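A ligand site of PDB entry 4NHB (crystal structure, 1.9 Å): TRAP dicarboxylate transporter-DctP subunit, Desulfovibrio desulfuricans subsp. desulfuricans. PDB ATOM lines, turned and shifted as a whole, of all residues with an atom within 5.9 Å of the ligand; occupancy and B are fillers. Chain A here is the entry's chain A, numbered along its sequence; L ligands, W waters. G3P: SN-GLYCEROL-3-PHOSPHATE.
The guanidinium group of Arg 171 is in hydrogen-bond range of the backbone carbonyl oxygen of Met 192, at 2.9 Å.
The side-chain hydroxyl (OH) of Tyr 178 is in hydrogen-bond range of the side-chain carboxylate (OE1) of Glu 107 (2.7 Å).
The guanidinium group of Arg 151 is in hydrogen-bond range of the side-chain hydroxyl of Tyr 178, 2.9 Å away.
NE of Arg 151 lies within salt-bridge range of OD2 of Asp 210, 2.9 Å away.
The side-chain sulfur (SD) of Met 36 lies within hydrogen-bond range of the side-chain amide nitrogen (NE2) of Gln 95 (3.3 Å).
OE2 of Glu 75 sits at hydrogen-bond distance from NE2 of Gln 95 (2.8 Å).
OG1 of Thr 92 lies within hydrogen-bond range of OE1 of Gln 95 (3.3 Å).
N of Leu 148 sits at hydrogen-bond distance from O of Val 236.
Water W2 lies within hydrogen-bond range of O3P of the ligand (2.5 Å), OD2 of Asp 215 (2.7 Å) and OG of Ser 211 (2.8 Å).
Water W1 lies within hydrogen-bond range of the side-chain carboxylate (OE2) of Glu 75, an oxygen (O2P) of the ligand and the backbone NH (N) of Phe 194.
Met 36 touches the ligand.
CA of Gly 93 touches O1 of the ligand, at 3.4 Å.
Pro 173 touches the ligand.
CD1 of Ile 175 touches C1 of the ligand (3.7 Å).
Phe 194 touches the ligand (CD1 to O3P, 3.6 Å).
CG1 of Val 236 touches O1 of the ligand, 3.96 Å away.
Hydrophobic or aromatic side chains within 4 Å of the ligand: Met 36, Pro 173, Ile 175, Phe 194, Val 236 and His 238.
Of the 24 residues printed, 13 come within 4 Å of the ligand.
The nearest printed residue that does not touch the ligand is Ile 237 (4.1 Å).
NZ of Lys 37 lies within salt-bridge range of O4P of the ligand (2.7 Å).
NH1 of Arg 171 is in salt-bridge range of O3P of the ligand (2.7 Å).
NE2 of His 238 is in hydrogen-bond range of O2 of the ligand (2.7 Å).
The side-chain carboxylate of Glu 107 is in hydrogen-bond range of an oxygen (O1) of the ligand (2.7 Å).
An oxygen (O3P) of the ligand lies within salt-bridge range of the guanidinium group (NH1) of Arg 151.
An oxygen (O1) of the ligand is in hydrogen-bond range of the backbone NH (N) of Thr 94 (3.1 Å).
An oxygen (O1) of the ligand sits close to the side-chain hydroxyl (OG1) of Thr 94, at 3.4 Å.
An oxygen (O2) of the ligand lies within hydrogen-bond range of the side-chain amide nitrogen (NE2) of Gln 95, at 3.4 Å.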
ATOM      1  N   MET A  36     -11.822 -20.978  -7.258  1.00  0.00           N
ATOM      2  CA  MET A  36     -11.228 -20.677  -5.954  1.00  0.00           C
ATOM      3  C   MET A  36     -12.295 -20.406  -4.927  1.00  0.00           C
ATOM      4  O   MET A  36     -11.968 -20.123  -3.768  1.00  0.00           O
ATOM      5  CB  MET A  36     -10.276 -19.465  -6.044  1.00  0.00           C
ATOM      6  CG  MET A  36     -10.985 -18.174  -6.425  1.00  0.00           C
ATOM      7  SD  MET A  36      -9.843 -16.722  -6.409  1.00  0.00           S
ATOM      8  CE  MET A  36      -9.624 -16.501  -4.635  1.00  0.00           C
ATOM      9  N   LYS A  37     -13.569 -20.519  -5.334  1.00  0.00           N
ATOM     10  CA  LYS A  37     -14.685 -20.130  -4.460  1.00  0.00           C
ATOM     11  C   LYS A  37     -15.621 -21.290  -4.128  1.00  0.00           C
ATOM     12  O   LYS A  37     -15.703 -22.285  -4.865  1.00  0.00           O
ATOM     13  CB  LYS A  37     -15.472 -18.931  -5.015  1.00  0.00           C
ATOM     14  CG  LYS A  37     -14.691 -17.646  -5.248  1.00  0.00           C
ATOM     15  CD  LYS A  37     -14.071 -17.091  -3.935  1.00  0.00           C
ATOM     16  CE  LYS A  37     -13.230 -15.837  -4.212  1.00  0.00           C
ATOM     17  NZ  LYS A  37     -12.831 -15.123  -2.944  1.00  0.00           N
ATOM     18  N   GLU A  75      -4.915 -20.434  -6.598  1.00  0.00           N
ATOM     19  CA  GLU A  75      -4.880 -19.706  -7.878  1.00  0.00           C
ATOM     20  C   GLU A  75      -3.550 -19.882  -8.618  1.00  0.00           C
ATOM     21  O   GLU A  75      -3.529 -20.164  -9.796  1.00  0.00           O
ATOM     22  CB  GLU A  75      -5.123 -18.213  -7.672  1.00  0.00           C
ATOM     23  CG  GLU A  75      -6.469 -17.877  -6.993  1.00  0.00           C
ATOM     24  CD  GLU A  75      -6.324 -17.611  -5.510  1.00  0.00           C
ATOM     25  OE1 GLU A  75      -5.982 -18.545  -4.774  1.00  0.00           O
ATOM     26  OE2 GLU A  75      -6.534 -16.471  -5.055  1.00  0.00           O
ATOM     27  N   THR A  92     -10.787 -16.864 -12.223  1.00  0.00           N
ATOM     28  CA  THR A  92     -10.026 -16.136 -11.230  1.00  0.00           C
ATOM     29  C   THR A  92     -10.133 -14.645 -11.515  1.00  0.00           C
ATOM     30  O   THR A  92     -10.829 -14.237 -12.476  1.00  0.00           O
ATOM     31  CB  THR A  92      -8.566 -16.673 -11.165  1.00  0.00           C
ATOM     32  OG1 THR A  92      -7.948 -16.253  -9.951  1.00  0.00           O
ATOM     33  CG2 THR A  92      -7.712 -16.169 -12.317  1.00  0.00           C
ATOM     34  N   GLY A  93      -9.473 -13.847 -10.676  1.00  0.00           N
ATOM     35  CA  GLY A  93      -9.502 -12.414 -10.793  1.00  0.00           C
ATOM     36  C   GLY A  93      -8.149 -11.754 -11.056  1.00  0.00           C
ATOM     37  O   GLY A  93      -7.386 -12.156 -11.954  1.00  0.00           O
ATOM     38  N   THR A  94      -7.844 -10.711 -10.291  1.00  0.00           N
ATOM     39  CA  THR A  94      -6.649  -9.916 -10.570  1.00  0.00           C
ATOM     40  C   THR A  94      -5.338 -10.612 -10.147  1.00  0.00           C
ATOM     41  O   THR A  94      -4.244  -9.990 -10.169  1.00  0.00           O
ATOM     42  CB  THR A  94      -6.727  -8.550  -9.889  1.00  0.00           C
ATOM     43  OG1 THR A  94      -6.985  -8.754  -8.501  1.00  0.00           O
ATOM     44  CG2 THR A  94      -7.832  -7.663 -10.532  1.00  0.00           C
ATOM     45  N   GLN A  95      -5.461 -11.880  -9.756  1.00  0.00           N
ATOM     46  CA  GLN A  95      -4.312 -12.775  -9.619  1.00  0.00           C
ATOM     47  C   GLN A  95      -3.494 -12.772 -10.920  1.00  0.00           C
ATOM     48  O   GLN A  95      -2.274 -12.910 -10.924  1.00  0.00           O
ATOM     49  CB  GLN A  95      -4.782 -14.192  -9.276  1.00  0.00           C
ATOM     50  CG  GLN A  95      -5.407 -14.393  -7.854  1.00  0.00           C
ATOM     51  CD  GLN A  95      -6.893 -13.976  -7.766  1.00  0.00           C
ATOM     52  OE1 GLN A  95      -7.420 -13.275  -8.649  1.00  0.00           O
ATOM     53  NE2 GLN A  95      -7.556 -14.409  -6.720  1.00  0.00           N
ATOM     54  N   GLU A 107      -9.717  -4.105 -10.947  1.00  0.00           N
ATOM     55  CA  GLU A 107     -10.142  -3.786  -9.580  1.00  0.00           C
ATOM     56  C   GLU A 107      -9.550  -2.458  -9.025  1.00  0.00           C
ATOM     57  O   GLU A 107      -9.281  -2.346  -7.845  1.00  0.00           O
ATOM     58  CB  GLU A 107      -9.831  -4.997  -8.656  1.00  0.00           C
ATOM     59  CG  GLU A 107     -10.595  -6.234  -9.043  1.00  0.00           C
ATOM     60  CD  GLU A 107     -10.362  -7.445  -8.162  1.00  0.00           C
ATOM     61  OE1 GLU A 107      -9.331  -7.504  -7.442  1.00  0.00           O
ATOM     62  OE2 GLU A 107     -11.221  -8.377  -8.211  1.00  0.00           O
ATOM     63  N   LEU A 148     -17.945 -10.128  -8.262  1.00  0.00           N
ATOM     64  CA  LEU A 148     -18.183 -10.871  -7.037  1.00  0.00           C
ATOM     65  C   LEU A 148     -18.766  -9.928  -5.973  1.00  0.00           C
ATOM     66  O   LEU A 148     -19.384 -10.383  -4.996  1.00  0.00           O
ATOM     67  CB  LEU A 148     -16.911 -11.590  -6.541  1.00  0.00           C
ATOM     68  CG  LEU A 148     -16.570 -12.987  -7.118  1.00  0.00           C
ATOM     69  CD1 LEU A 148     -16.564 -13.041  -8.608  1.00  0.00           C
ATOM     70  CD2 LEU A 148     -15.280 -13.567  -6.549  1.00  0.00           C
ATOM     71  N   ARG A 151     -16.102  -4.730  -1.917  1.00  0.00           N
ATOM     72  CA  ARG A 151     -15.455  -5.233  -0.676  1.00  0.00           C
ATOM     73  C   ARG A 151     -15.831  -4.354   0.510  1.00  0.00           C
ATOM     74  O   ARG A 151     -15.785  -3.128   0.399  1.00  0.00           O
ATOM     75  CB  ARG A 151     -13.928  -5.277  -0.817  1.00  0.00           C
ATOM     76  CG  ARG A 151     -13.427  -6.039  -2.086  1.00  0.00           C
ATOM     77  CD  ARG A 151     -11.921  -6.297  -2.070  1.00  0.00           C
ATOM     78  NE  ARG A 151     -11.537  -7.326  -1.112  1.00  0.00           N
ATOM     79  CZ  ARG A 151     -11.093  -8.543  -1.417  1.00  0.00           C
ATOM     80  NH1 ARG A 151     -10.821  -9.403  -0.464  1.00  0.00           N
ATOM     81  NH2 ARG A 151     -10.918  -8.921  -2.674  1.00  0.00           N
ATOM     82  N   ARG A 171      -6.359  -9.532   7.266  1.00  0.00           N
ATOM     83  CA  ARG A 171      -6.062 -10.341   6.087  1.00  0.00           C
ATOM     84  C   ARG A 171      -6.111  -9.478   4.842  1.00  0.00           C
ATOM     85  O   ARG A 171      -6.947  -8.599   4.719  1.00  0.00           O
ATOM     86  CB  ARG A 171      -7.071 -11.469   5.951  1.00  0.00           C
ATOM     87  CG  ARG A 171      -6.717 -12.438   4.815  1.00  0.00           C
ATOM     88  CD  ARG A 171      -7.629 -12.214   3.582  1.00  0.00           C
ATOM     89  NE  ARG A 171      -7.131 -12.876   2.382  1.00  0.00           N
ATOM     90  CZ  ARG A 171      -7.822 -13.019   1.253  1.00  0.00           C
ATOM     91  NH1 ARG A 171      -9.052 -12.527   1.160  1.00  0.00           N
ATOM     92  NH2 ARG A 171      -7.287 -13.618   0.226  1.00  0.00           N
ATOM     93  N   PRO A 173      -5.462 -10.210   0.397  1.00  0.00           N
ATOM     94  CA  PRO A 173      -5.045 -11.140  -0.652  1.00  0.00           C
ATOM     95  C   PRO A 173      -3.579 -10.899  -0.984  1.00  0.00           C
ATOM     96  O   PRO A 173      -3.140  -9.755  -0.850  1.00  0.00           O
ATOM     97  CB  PRO A 173      -5.908 -10.738  -1.845  1.00  0.00           C
ATOM     98  CG  PRO A 173      -7.178 -10.220  -1.245  1.00  0.00           C
ATOM     99  CD  PRO A 173      -6.647  -9.435  -0.005  1.00  0.00           C
ATOM    100  N   ILE A 175      -1.745 -10.203  -3.534  1.00  0.00           N
ATOM    101  CA  ILE A 175      -1.746  -9.648  -4.870  1.00  0.00           C
ATOM    102  C   ILE A 175      -1.277  -8.216  -4.695  1.00  0.00           C
ATOM    103  O   ILE A 175      -1.694  -7.557  -3.762  1.00  0.00           O
ATOM    104  CB  ILE A 175      -3.201  -9.636  -5.486  1.00  0.00           C
ATOM    105  CG1 ILE A 175      -3.825 -11.037  -5.487  1.00  0.00           C
ATOM    106  CG2 ILE A 175      -3.172  -9.049  -6.887  1.00  0.00           C
ATOM    107  CD1 ILE A 175      -5.281 -11.104  -6.070  1.00  0.00           C
ATOM    108  N   TYR A 178      -3.626  -5.180  -3.684  1.00  0.00           N
ATOM    109  CA  TYR A 178      -4.190  -5.254  -2.321  1.00  0.00           C
ATOM    110  C   TYR A 178      -3.191  -4.940  -1.156  1.00  0.00           C
ATOM    111  O   TYR A 178      -3.537  -4.286  -0.183  1.00  0.00           O
ATOM    112  CB  TYR A 178      -4.795  -6.655  -2.099  1.00  0.00           C
ATOM    113  CG  TYR A 178      -6.114  -6.842  -2.817  1.00  0.00           C
ATOM    114  CD1 TYR A 178      -7.283  -6.412  -2.259  1.00  0.00           C
ATOM    115  CD2 TYR A 178      -6.174  -7.411  -4.091  1.00  0.00           C
ATOM    116  CE1 TYR A 178      -8.509  -6.572  -2.921  1.00  0.00           C
ATOM    117  CE2 TYR A 178      -7.393  -7.544  -4.762  1.00  0.00           C
ATOM    118  CZ  TYR A 178      -8.539  -7.147  -4.145  1.00  0.00           C
ATOM    119  OH  TYR A 178      -9.756  -7.259  -4.786  1.00  0.00           O
ATOM    120  N   MET A 192      -2.520 -13.636   2.538  1.00  0.00           N
ATOM    121  CA  MET A 192      -2.733 -15.062   2.433  1.00  0.00           C
ATOM    122  C   MET A 192      -3.785 -15.390   1.367  1.00  0.00           C
ATOM    123  O   MET A 192      -4.757 -14.631   1.180  1.00  0.00           O
ATOM    124  CB  MET A 192      -3.156 -15.625   3.767  1.00  0.00           C
ATOM    125  CG  MET A 192      -4.516 -15.176   4.220  1.00  0.00           C
ATOM    126  SD  MET A 192      -4.871 -15.740   5.895  1.00  0.00           S
ATOM    127  CE  MET A 192      -3.955 -14.593   6.907  1.00  0.00           C
ATOM    128  N   PRO A 193      -3.599 -16.508   0.635  1.00  0.00           N
ATOM    129  CA  PRO A 193      -4.662 -16.922  -0.285  1.00  0.00           C
ATOM    130  C   PRO A 193      -6.034 -17.075   0.381  1.00  0.00           C
ATOM    131  O   PRO A 193      -6.163 -17.370   1.569  1.00  0.00           O
ATOM    132  CB  PRO A 193      -4.182 -18.285  -0.804  1.00  0.00           C
ATOM    133  CG  PRO A 193      -2.725 -18.257  -0.624  1.00  0.00           C
ATOM    134  CD  PRO A 193      -2.404 -17.343   0.513  1.00  0.00           C
ATOM    135  N   PHE A 194      -7.066 -16.915  -0.435  1.00  0.00           N
ATOM    136  CA  PHE A 194      -8.424 -17.033   0.068  1.00  0.00           C
ATOM    137  C   PHE A 194      -8.699 -18.380   0.794  1.00  0.00           C
ATOM    138  O   PHE A 194      -9.389 -18.429   1.820  1.00  0.00           O
ATOM    139  CB  PHE A 194      -9.393 -16.893  -1.094  1.00  0.00           C
ATOM    140  CG  PHE A 194     -10.807 -16.829  -0.653  1.00  0.00           C
ATOM    141  CD1 PHE A 194     -11.266 -15.701   0.024  1.00  0.00           C
ATOM    142  CD2 PHE A 194     -11.673 -17.901  -0.866  1.00  0.00           C
ATOM    143  CE1 PHE A 194     -12.584 -15.631   0.470  1.00  0.00           C
ATOM    144  CE2 PHE A 194     -12.988 -17.839  -0.408  1.00  0.00           C
ATOM    145  CZ  PHE A 194     -13.447 -16.718   0.238  1.00  0.00           C
ATOM    146  N   ASP A 210     -11.190  -7.526   4.446  1.00  0.00           N
ATOM    147  CA  ASP A 210     -12.332  -6.990   3.722  1.00  0.00           C
ATOM    148  C   ASP A 210     -12.591  -7.943   2.551  1.00  0.00           C
ATOM    149  O   ASP A 210     -11.641  -8.408   1.903  1.00  0.00           O
ATOM    150  CB  ASP A 210     -12.069  -5.586   3.177  1.00  0.00           C
ATOM    151  CG  ASP A 210     -10.882  -5.528   2.266  1.00  0.00           C
ATOM    152  OD1 ASP A 210      -9.730  -5.525   2.778  1.00  0.00           O
ATOM    153  OD2 ASP A 210     -11.044  -5.457   1.026  1.00  0.00           O
ATOM    154  N   SER A 211     -13.865  -8.216   2.315  1.00  0.00           N
ATOM    155  CA  SER A 211     -14.322  -9.160   1.298  1.00  0.00           C
ATOM    156  C   SER A 211     -15.643  -8.711   0.735  1.00  0.00           C
ATOM    157  O   SER A 211     -16.376  -7.952   1.370  1.00  0.00           O
ATOM    158  CB  SER A 211     -14.497 -10.543   1.886  1.00  0.00           C
ATOM    159  OG  SER A 211     -13.260 -11.217   2.081  1.00  0.00           O
ATOM    160  N   PRO A 212     -15.986  -9.212  -0.474  1.00  0.00           N
ATOM    161  CA  PRO A 212     -17.376  -9.076  -0.900  1.00  0.00           C
ATOM    162  C   PRO A 212     -18.338  -9.739   0.092  1.00  0.00           C
ATOM    163  O   PRO A 212     -17.950 -10.701   0.780  1.00  0.00           O
ATOM    164  CB  PRO A 212     -17.413  -9.842  -2.244  1.00  0.00           C
ATOM    165  CG  PRO A 212     -16.005  -9.868  -2.719  1.00  0.00           C
ATOM    166  CD  PRO A 212     -15.148  -9.926  -1.455  1.00  0.00           C
ATOM    167  N   ASP A 215     -18.693 -13.515   0.056  1.00  0.00           N
ATOM    168  CA  ASP A 215     -17.657 -14.298   0.718  1.00  0.00           C
ATOM    169  C   ASP A 215     -17.837 -14.223   2.233  1.00  0.00           C
ATOM    170  O   ASP A 215     -17.708 -15.235   2.944  1.00  0.00           O
ATOM    171  CB  ASP A 215     -16.265 -13.813   0.264  1.00  0.00           C
ATOM    172  CG  ASP A 215     -15.915 -14.255  -1.150  1.00  0.00           C
ATOM    173  OD1 ASP A 215     -16.657 -15.106  -1.699  1.00  0.00           O
ATOM    174  OD2 ASP A 215     -14.869 -13.733  -1.701  1.00  0.00           O
ATOM    175  N   VAL A 236     -14.753  -6.442  -6.668  1.00  0.00           N
ATOM    176  CA  VAL A 236     -14.115  -7.609  -7.182  1.00  0.00           C
ATOM    177  C   VAL A 236     -14.709  -8.017  -8.524  1.00  0.00           C
ATOM    178  O   VAL A 236     -15.915  -8.151  -8.684  1.00  0.00           O
ATOM    179  CB  VAL A 236     -14.166  -8.797  -6.151  1.00  0.00           C
ATOM    180  CG1 VAL A 236     -13.485 -10.086  -6.679  1.00  0.00           C
ATOM    181  CG2 VAL A 236     -13.537  -8.373  -4.841  1.00  0.00           C
ATOM    182  N   ILE A 237     -13.821  -8.202  -9.499  1.00  0.00           N
ATOM    183  CA  ILE A 237     -14.185  -8.626 -10.850  1.00  0.00           C
ATOM    184  C   ILE A 237     -13.406  -9.891 -11.187  1.00  0.00           C
ATOM    185  O   ILE A 237     -12.172  -9.903 -11.108  1.00  0.00           O
ATOM    186  CB  ILE A 237     -13.809  -7.543 -11.861  1.00  0.00           C
ATOM    187  CG1 ILE A 237     -14.629  -6.255 -11.630  1.00  0.00           C
ATOM    188  CG2 ILE A 237     -13.978  -8.063 -13.301  1.00  0.00           C
ATOM    189  CD1 ILE A 237     -16.128  -6.375 -11.985  1.00  0.00           C
ATOM    190  N   HIS A 238     -14.104 -10.975 -11.529  1.00  0.00           N
ATOM    191  CA  HIS A 238     -13.418 -12.172 -12.049  1.00  0.00           C
ATOM    192  C   HIS A 238     -13.751 -12.463 -13.510  1.00  0.00           C
ATOM    193  O   HIS A 238     -14.604 -11.812 -14.108  1.00  0.00           O
ATOM    194  CB  HIS A 238     -13.768 -13.365 -11.172  1.00  0.00           C
ATOM    195  CG  HIS A 238     -13.010 -13.414  -9.895  1.00  0.00           C
ATOM    196  ND1 HIS A 238     -12.829 -14.592  -9.205  1.00  0.00           N
ATOM    197  CD2 HIS A 238     -12.366 -12.447  -9.190  1.00  0.00           C
ATOM    198  CE1 HIS A 238     -12.112 -14.353  -8.114  1.00  0.00           C
ATOM    199  NE2 HIS A 238     -11.837 -13.058  -8.071  1.00  0.00           N
HETATM  200  O1  G3P L   1      -9.759 -10.667  -7.881  1.00  0.00           O
HETATM  201  C1  G3P L   1      -8.912 -10.793  -6.784  1.00  0.00           C
HETATM  202  C2  G3P L   1      -9.697 -11.323  -5.571  1.00  0.00           C
HETATM  203  O2  G3P L   1     -10.271 -12.564  -5.895  1.00  0.00           O
HETATM  204  C3  G3P L   1      -8.755 -11.473  -4.374  1.00  0.00           C
HETATM  205  O1P G3P L   1      -9.483 -11.368  -3.197  1.00  0.00           O
HETATM  206  O4P G3P L   1     -10.855 -13.367  -3.414  1.00  0.00           O
HETATM  207  O2P G3P L   1      -8.613 -13.525  -2.214  1.00  0.00           O
HETATM  208  O3P G3P L   1     -10.528 -12.375  -1.106  1.00  0.00           O
HETATM  209  P   G3P L   1      -9.882 -12.745  -2.442  1.00  0.00           P
HETATM  210  O   HOH W   1      -6.625 -15.144  -2.883  1.00  0.00           O
HETATM  211  O   HOH W   2     -12.891 -12.364  -0.415  1.00  0.00           O
